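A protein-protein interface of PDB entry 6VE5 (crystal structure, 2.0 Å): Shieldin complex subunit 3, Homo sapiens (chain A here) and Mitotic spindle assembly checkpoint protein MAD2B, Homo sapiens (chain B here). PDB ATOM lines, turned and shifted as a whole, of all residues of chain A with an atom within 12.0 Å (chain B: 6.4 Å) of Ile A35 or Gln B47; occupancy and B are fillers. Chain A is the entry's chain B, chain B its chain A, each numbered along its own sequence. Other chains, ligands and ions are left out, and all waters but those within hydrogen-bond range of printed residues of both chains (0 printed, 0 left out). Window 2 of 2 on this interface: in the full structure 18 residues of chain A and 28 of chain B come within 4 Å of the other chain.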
ATOM      1  N   ILE A  21       8.950 -20.899 -19.359  1.00  0.00           N
ATOM      2  CA  ILE A  21       9.993 -21.421 -18.483  1.00  0.00           C
ATOM      3  C   ILE A  21      10.352 -22.817 -18.969  1.00  0.00           C
ATOM      4  O   ILE A  21       9.573 -23.766 -18.796  1.00  0.00           O
ATOM      5  CB  ILE A  21       9.560 -21.439 -17.013  1.00  0.00           C
ATOM      6  CG1 ILE A  21       9.265 -20.006 -16.543  1.00  0.00           C
ATOM      7  CG2 ILE A  21      10.641 -22.078 -16.151  1.00  0.00           C
ATOM      8  CD1 ILE A  21       8.754 -19.915 -15.129  1.00  0.00           C
ATOM      9  N   ALA A  25      15.709 -23.865 -17.668  1.00  0.00           N
ATOM     10  CA  ALA A  25      15.669 -22.695 -16.799  1.00  0.00           C
ATOM     11  C   ALA A  25      15.201 -23.063 -15.399  1.00  0.00           C
ATOM     12  O   ALA A  25      15.636 -22.448 -14.419  1.00  0.00           O
ATOM     13  CB  ALA A  25      14.764 -21.624 -17.401  1.00  0.00           C
ATOM     14  N   ALA A  26      14.331 -24.070 -15.285  1.00  0.00           N
ATOM     15  CA  ALA A  26      13.852 -24.496 -13.975  1.00  0.00           C
ATOM     16  C   ALA A  26      14.979 -25.075 -13.135  1.00  0.00           C
ATOM     17  O   ALA A  26      15.035 -24.847 -11.922  1.00  0.00           O
ATOM     18  CB  ALA A  26      12.731 -25.520 -14.134  1.00  0.00           C
ATOM     19  N   GLU A  27      15.884 -25.835 -13.756  1.00  0.00           N
ATOM     20  CA  GLU A  27      17.012 -26.382 -13.014  1.00  0.00           C
ATOM     21  C   GLU A  27      17.907 -25.269 -12.487  1.00  0.00           C
ATOM     22  O   GLU A  27      18.416 -25.351 -11.364  1.00  0.00           O
ATOM     23  CB  GLU A  27      17.806 -27.344 -13.899  1.00  0.00           C
ATOM     24  CG  GLU A  27      17.118 -28.682 -14.124  1.00  0.00           C
ATOM     25  CD  GLU A  27      17.069 -29.536 -12.869  1.00  0.00           C
ATOM     26  OE1 GLU A  27      17.616 -29.107 -11.830  1.00  0.00           O
ATOM     27  OE2 GLU A  27      16.488 -30.642 -12.924  1.00  0.00           O
ATOM     28  N   ASP A  28      18.108 -24.216 -13.279  1.00  0.00           N
ATOM     29  CA  ASP A  28      18.872 -23.070 -12.800  1.00  0.00           C
ATOM     30  C   ASP A  28      18.204 -22.444 -11.583  1.00  0.00           C
ATOM     31  O   ASP A  28      18.872 -22.131 -10.591  1.00  0.00           O
ATOM     32  CB  ASP A  28      19.036 -22.043 -13.919  1.00  0.00           C
ATOM     33  CG  ASP A  28      19.952 -22.529 -15.028  1.00  0.00           C
ATOM     34  OD1 ASP A  28      20.884 -23.305 -14.731  1.00  0.00           O
ATOM     35  OD2 ASP A  28      19.743 -22.138 -16.195  1.00  0.00           O
ATOM     36  N   VAL A  29      16.882 -22.262 -11.637  1.00  0.00           N
ATOM     37  CA  VAL A  29      16.163 -21.683 -10.506  1.00  0.00           C
ATOM     38  C   VAL A  29      16.323 -22.564  -9.275  1.00  0.00           C
ATOM     39  O   VAL A  29      16.636 -22.083  -8.179  1.00  0.00           O
ATOM     40  CB  VAL A  29      14.680 -21.480 -10.865  1.00  0.00           C
ATOM     41  CG1 VAL A  29      13.886 -21.005  -9.649  1.00  0.00           C
ATOM     42  CG2 VAL A  29      14.544 -20.497 -12.009  1.00  0.00           C
ATOM     43  N   LYS A  30      16.118 -23.875  -9.444  1.00  0.00           N
ATOM     44  CA  LYS A  30      16.228 -24.796  -8.318  1.00  0.00           C
ATOM     45  C   LYS A  30      17.632 -24.793  -7.729  1.00  0.00           C
ATOM     46  O   LYS A  30      17.799 -24.982  -6.520  1.00  0.00           O
ATOM     47  CB  LYS A  30      15.848 -26.207  -8.764  1.00  0.00           C
ATOM     48  CG  LYS A  30      15.654 -27.195  -7.624  1.00  0.00           C
ATOM     49  CD  LYS A  30      15.331 -28.589  -8.149  1.00  0.00           C
ATOM     50  CE  LYS A  30      14.856 -29.512  -7.036  1.00  0.00           C
ATOM     51  NZ  LYS A  30      15.896 -29.723  -5.990  1.00  0.00           N
ATOM     52  N   GLN A  31      18.649 -24.572  -8.563  1.00  0.00           N
ATOM     53  CA  GLN A  31      20.029 -24.650  -8.100  1.00  0.00           C
ATOM     54  C   GLN A  31      20.422 -23.421  -7.287  1.00  0.00           C
ATOM     55  O   GLN A  31      20.996 -23.546  -6.200  1.00  0.00           O
ATOM     56  CB  GLN A  31      20.963 -24.822  -9.302  1.00  0.00           C
ATOM     57  CG  GLN A  31      22.423 -25.044  -8.945  1.00  0.00           C
ATOM     58  CD  GLN A  31      23.289 -25.299 -10.166  1.00  0.00           C
ATOM     59  OE1 GLN A  31      22.783 -25.524 -11.267  1.00  0.00           O
ATOM     60  NE2 GLN A  31      24.602 -25.263  -9.977  1.00  0.00           N
ATOM     61  N   TYR A  32      20.104 -22.226  -7.785  1.00  0.00           N
ATOM     62  CA  TYR A  32      20.625 -20.994  -7.204  1.00  0.00           C
ATOM     63  C   TYR A  32      19.622 -20.227  -6.358  1.00  0.00           C
ATOM     64  O   TYR A  32      20.036 -19.490  -5.455  1.00  0.00           O
ATOM     65  CB  TYR A  32      21.131 -20.060  -8.314  1.00  0.00           C
ATOM     66  CG  TYR A  32      22.249 -20.639  -9.143  1.00  0.00           C
ATOM     67  CD1 TYR A  32      23.568 -20.552  -8.719  1.00  0.00           C
ATOM     68  CD2 TYR A  32      21.988 -21.270 -10.351  1.00  0.00           C
ATOM     69  CE1 TYR A  32      24.597 -21.081  -9.469  1.00  0.00           C
ATOM     70  CE2 TYR A  32      23.017 -21.808 -11.113  1.00  0.00           C
ATOM     71  CZ  TYR A  32      24.318 -21.708 -10.664  1.00  0.00           C
ATOM     72  OH  TYR A  32      25.347 -22.234 -11.409  1.00  0.00           O
ATOM     73  N   LEU A  33      18.321 -20.371  -6.617  1.00  0.00           N
ATOM     74  CA  LEU A  33      17.323 -19.476  -6.048  1.00  0.00           C
ATOM     75  C   LEU A  33      16.412 -20.160  -5.035  1.00  0.00           C
ATOM     76  O   LEU A  33      15.365 -19.611  -4.684  1.00  0.00           O
ATOM     77  CB  LEU A  33      16.489 -18.851  -7.169  1.00  0.00           C
ATOM     78  CG  LEU A  33      17.295 -18.172  -8.278  1.00  0.00           C
ATOM     79  CD1 LEU A  33      16.369 -17.533  -9.307  1.00  0.00           C
ATOM     80  CD2 LEU A  33      18.247 -17.134  -7.703  1.00  0.00           C
ATOM     81  N   THR A  34      16.790 -21.338  -4.548  1.00  0.00           N
ATOM     82  CA  THR A  34      16.027 -22.034  -3.524  1.00  0.00           C
ATOM     83  C   THR A  34      16.887 -22.229  -2.282  1.00  0.00           C
ATOM     84  O   THR A  34      18.117 -22.149  -2.332  1.00  0.00           O
ATOM     85  CB  THR A  34      15.517 -23.389  -4.028  1.00  0.00           C
ATOM     86  OG1 THR A  34      16.627 -24.241  -4.329  1.00  0.00           O
ATOM     87  CG2 THR A  34      14.667 -23.200  -5.279  1.00  0.00           C
ATOM     88  N   ILE A  35      16.221 -22.488  -1.162  1.00  0.00           N
ATOM     89  CA  ILE A  35      16.897 -22.603   0.123  1.00  0.00           C
ATOM     90  C   ILE A  35      17.120 -24.072   0.468  1.00  0.00           C
ATOM     91  O   ILE A  35      16.411 -24.952  -0.023  1.00  0.00           O
ATOM     92  CB  ILE A  35      16.097 -21.880   1.227  1.00  0.00           C
ATOM     93  CG1 ILE A  35      17.046 -21.177   2.202  1.00  0.00           C
ATOM     94  CG2 ILE A  35      15.193 -22.855   1.977  1.00  0.00           C
ATOM     95  CD1 ILE A  35      17.694 -19.932   1.631  1.00  0.00           C
ATOM     96  N   VAL B  43       8.030 -28.139 -12.102  1.00  0.00           N
ATOM     97  CA  VAL B  43       7.990 -28.153 -10.639  1.00  0.00           C
ATOM     98  C   VAL B  43       9.262 -27.570 -10.038  1.00  0.00           C
ATOM     99  O   VAL B  43       9.251 -27.066  -8.908  1.00  0.00           O
ATOM    100  CB  VAL B  43       7.750 -29.594 -10.146  1.00  0.00           C
ATOM    101  CG1 VAL B  43       8.163 -29.746  -8.690  1.00  0.00           C
ATOM    102  CG2 VAL B  43       6.291 -29.979 -10.332  1.00  0.00           C
ATOM    103  N   GLY B  44      10.372 -27.618 -10.773  1.00  0.00           N
ATOM    104  CA  GLY B  44      11.654 -27.243 -10.203  1.00  0.00           C
ATOM    105  C   GLY B  44      11.721 -25.815  -9.700  1.00  0.00           C
ATOM    106  O   GLY B  44      12.522 -25.498  -8.819  1.00  0.00           O
ATOM    107  N   ILE B  45      10.881 -24.926 -10.248  1.00  0.00           N
ATOM    108  CA  ILE B  45      10.939 -23.518  -9.862  1.00  0.00           C
ATOM    109  C   ILE B  45      10.309 -23.247  -8.509  1.00  0.00           C
ATOM    110  O   ILE B  45      10.495 -22.154  -7.952  1.00  0.00           O
ATOM    111  CB  ILE B  45      10.239 -22.609 -10.892  1.00  0.00           C
ATOM    112  CG1 ILE B  45       8.727 -22.850 -10.907  1.00  0.00           C
ATOM    113  CG2 ILE B  45      10.813 -22.843 -12.282  1.00  0.00           C
ATOM    114  CD1 ILE B  45       7.960 -21.859 -11.785  1.00  0.00           C
ATOM    115  N   PHE B  46       9.561 -24.200  -7.966  1.00  0.00           N
ATOM    116  CA  PHE B  46       8.787 -23.964  -6.759  1.00  0.00           C
ATOM    117  C   PHE B  46       9.561 -24.381  -5.515  1.00  0.00           C
ATOM    118  O   PHE B  46      10.328 -25.344  -5.527  1.00  0.00           O
ATOM    119  CB  PHE B  46       7.460 -24.719  -6.821  1.00  0.00           C
ATOM    120  CG  PHE B  46       6.528 -24.214  -7.873  1.00  0.00           C
ATOM    121  CD1 PHE B  46       5.676 -23.159  -7.608  1.00  0.00           C
ATOM    122  CD2 PHE B  46       6.499 -24.791  -9.132  1.00  0.00           C
ATOM    123  CE1 PHE B  46       4.811 -22.688  -8.576  1.00  0.00           C
ATOM    124  CE2 PHE B  46       5.637 -24.320 -10.105  1.00  0.00           C
ATOM    125  CZ  PHE B  46       4.793 -23.262  -9.819  1.00  0.00           C
ATOM    126  N   GLN B  47       9.346 -23.633  -4.437  1.00  0.00           N
ATOM    127  CA  GLN B  47       9.942 -23.918  -3.139  1.00  0.00           C
ATOM    128  C   GLN B  47       8.839 -23.918  -2.091  1.00  0.00           C
ATOM    129  O   GLN B  47       8.034 -22.982  -2.027  1.00  0.00           O
ATOM    130  CB  GLN B  47      11.017 -22.878  -2.805  1.00  0.00           C
ATOM    131  CG  GLN B  47      11.276 -22.683  -1.323  1.00  0.00           C
ATOM    132  CD  GLN B  47      12.515 -21.847  -1.051  1.00  0.00           C
ATOM    133  OE1 GLN B  47      13.189 -22.033  -0.040  1.00  0.00           O
ATOM    134  NE2 GLN B  47      12.818 -20.921  -1.953  1.00  0.00           N
ATOM    135  N   LYS B  48       8.796 -24.966  -1.278  1.00  0.00           N
ATOM    136  CA  LYS B  48       7.747 -25.077  -0.273  1.00  0.00           C
ATOM    137  C   LYS B  48       7.965 -24.045   0.825  1.00  0.00           C
ATOM    138  O   LYS B  48       9.087 -23.838   1.295  1.00  0.00           O
ATOM    139  CB  LYS B  48       7.713 -26.488   0.318  1.00  0.00           C
ATOM    140  CG  LYS B  48       6.412 -26.809   1.045  1.00  0.00           C
ATOM    141  CD  LYS B  48       6.165 -28.310   1.142  1.00  0.00           C
ATOM    142  CE  LYS B  48       6.960 -28.951   2.269  1.00  0.00           C
ATOM    143  NZ  LYS B  48       6.787 -30.431   2.291  1.00  0.00           N
ATOM    144  N   ARG B  49       6.882 -23.387   1.224  1.00  0.00           N
ATOM    145  CA  ARG B  49       6.927 -22.336   2.223  1.00  0.00           C
ATOM    146  C   ARG B  49       5.669 -22.424   3.080  1.00  0.00           C
ATOM    147  O   ARG B  49       4.812 -23.293   2.879  1.00  0.00           O
ATOM    148  CB  ARG B  49       7.064 -20.961   1.559  1.00  0.00           C
ATOM    149  CG  ARG B  49       8.428 -20.323   1.743  1.00  0.00           C
ATOM    150  CD  ARG B  49       8.565 -19.063   0.909  1.00  0.00           C
ATOM    151  NE  ARG B  49       9.323 -19.301  -0.316  1.00  0.00           N
ATOM    152  CZ  ARG B  49       9.520 -18.391  -1.266  1.00  0.00           C
ATOM    153  NH1 ARG B  49       9.008 -17.174  -1.140  1.00  0.00           N
ATOM    154  NH2 ARG B  49      10.226 -18.699  -2.344  1.00  0.00           N
ATOM    155  N   VAL B  56       2.528 -24.149   1.377  1.00  0.00           N
ATOM    156  CA  VAL B  56       2.296 -23.536   0.076  1.00  0.00           C
ATOM    157  C   VAL B  56       3.513 -23.791  -0.804  1.00  0.00           C
ATOM    158  O   VAL B  56       4.560 -24.238  -0.340  1.00  0.00           O
ATOM    159  CB  VAL B  56       2.017 -22.021   0.182  1.00  0.00           C
ATOM    160  CG1 VAL B  56       0.712 -21.772   0.935  1.00  0.00           C
ATOM    161  CG2 VAL B  56       3.171 -21.316   0.862  1.00  0.00           C
ATOM    162  N   GLN B  57       3.362 -23.486  -2.089  1.00  0.00           N
ATOM    163  CA  GLN B  57       4.427 -23.637  -3.069  1.00  0.00           C
ATOM    164  C   GLN B  57       4.600 -22.309  -3.792  1.00  0.00           C
ATOM    165  O   GLN B  57       3.686 -21.861  -4.492  1.00  0.00           O
ATOM    166  CB  GLN B  57       4.108 -24.754  -4.064  1.00  0.00           C
ATOM    167  CG  GLN B  57       4.067 -26.136  -3.440  1.00  0.00           C
ATOM    168  CD  GLN B  57       5.446 -26.658  -3.093  1.00  0.00           C
ATOM    169  OE1 GLN B  57       6.448 -26.219  -3.658  1.00  0.00           O
ATOM    170  NE2 GLN B  57       5.506 -27.598  -2.157  1.00  0.00           N
ATOM    171  N   MET B  58       5.770 -21.692  -3.634  1.00  0.00           N
ATOM    172  CA  MET B  58       6.055 -20.386  -4.216  1.00  0.00           C
ATOM    173  C   MET B  58       7.105 -20.525  -5.310  1.00  0.00           C
ATOM    174  O   MET B  58       8.128 -21.189  -5.118  1.00  0.00           O
ATOM    175  CB  MET B  58       6.541 -19.401  -3.148  1.00  0.00           C
ATOM    176  CG  MET B  58       5.559 -19.157  -2.012  1.00  0.00           C
ATOM    177  SD  MET B  58       4.064 -18.284  -2.506  1.00  0.00           S
ATOM    178  CE  MET B  58       4.726 -16.721  -3.079  1.00  0.00           C
ATOM    179  N   SER B  59       6.842 -19.899  -6.451  1.00  0.00           N
ATOM    180  CA  SER B  59       7.820 -19.833  -7.524  1.00  0.00           C
ATOM    181  C   SER B  59       9.008 -18.971  -7.119  1.00  0.00           C
ATOM    182  O   SER B  59       8.857 -17.935  -6.468  1.00  0.00           O
ATOM    183  CB  SER B  59       7.169 -19.270  -8.795  1.00  0.00           C
ATOM    184  OG  SER B  59       8.123 -18.679  -9.665  1.00  0.00           O
ATOM    185  N   CYS B  60      10.203 -19.413  -7.506  1.00  0.00           N
ATOM    186  CA  CYS B  60      11.421 -18.634  -7.326  1.00  0.00           C
ATOM    187  C   CYS B  60      11.952 -18.108  -8.653  1.00  0.00           C
ATOM    188  O   CYS B  60      13.072 -17.591  -8.705  1.00  0.00           O
ATOM    189  CB  CYS B  60      12.482 -19.480  -6.625  1.00  0.00           C
ATOM    190  SG  CYS B  60      12.038 -19.918  -4.933  1.00  0.00           S
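NH2 of Arg B49 sits close to NE2 of Gln B47 (3.4 Å).
N of Gln B47 sits at hydrogen-bond distance from O of Met B58 (2.8 Å).
O of Lys A30 lies within hydrogen-bond range of OG1 of Thr A34 (2.6 Å).
The side-chain sulfur (SG) of Cys B60 is in hydrogen-bond range of the side-chain amide nitrogen (NE2) of Gln B47 (3.2 Å).
The backbone carbonyl oxygen (O) of Ile B45 sits at hydrogen-bond distance from the backbone NH (N) of Cys B60 (2.8 Å).
NH2 of Arg B49 lies within hydrogen-bond range of SG of Cys B60, 3.4 Å away.
Of the 12 printed residues of chain A, 7 touch a printed residue of chain B.
Of the 12 printed residues of chain B, 4 touch a printed residue of chain A.
Printed residues of chain B that touch a printed residue of chain A: Gly B44, Ile B45, Gln B47 and Cys B60.
Hydrophobic or aromatic side chains of chain B that line the printed part of chain A: Ile B45.
Among the printed residues, no Asp or Glu carboxylate lies within 4 Å of a Lys or Arg side-chain nitrogen of the other chain.
OE1 of Gln B47 sits close to N of Ile A35 (3.3 Å).
The side-chain sulfur of Cys B60 sits at hydrogen-bond distance from the backbone carbonyl oxygen of Leu A33 (3.4 Å).
Ile A21 touches Ile B45.
CG2 of Ile B45 touches CB of Ala A26, at 3.8 Å.
CA of Ile B45 touches CG1 of Val A29, 3.9 Å away.
C of Cys B60 touches CG1 of Val A29, 3.6 Å away.
Gly B44 touches Lys A30.
Gln B47 touches Leu A33.
Thr A34 touches Gln B47.
Printed residues of chain B within 4 Å of Ile A21: Ile B45 (3.9 Å).
Asp A28 touches none of the printed residues of chain B.
Of the printed residues of chain B, Leu A33 touches Gln B47 (3.96 Å) and Cys B60 (3.4 Å).
Printed residues of chain B within 4 Å of Ile A35: Gln B47.
Val B43 touches none of the printed residues of chain A.
Of the printed residues of chain A, Gly B44 touches Lys A30.
Of the printed residues of chain A, Ile B45 touches Ile A21, Ala A26 and Val A29.
Of chain A, only Leu A33 (3.96 Å), Thr A34 (3.7 Å) and Ile A35 (3.0 Å) come within 4 Å of Gln B47.
Arg B49 touches none of the printed residues of chain A.
No residue of chain A comes within 4 Å of Gln B57.
Met B58 touches none of the printed residues of chain A.
No residue of chain A comes within 4 Å of Ser B59.
Of chain A, only Val A29 (3.6 Å) and Leu A33 (3.4 Å) come within 4 Å of Cys B60.
The nearest residue of chain A that does not touch Gln B47 is Val A29 (7.4 Å).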
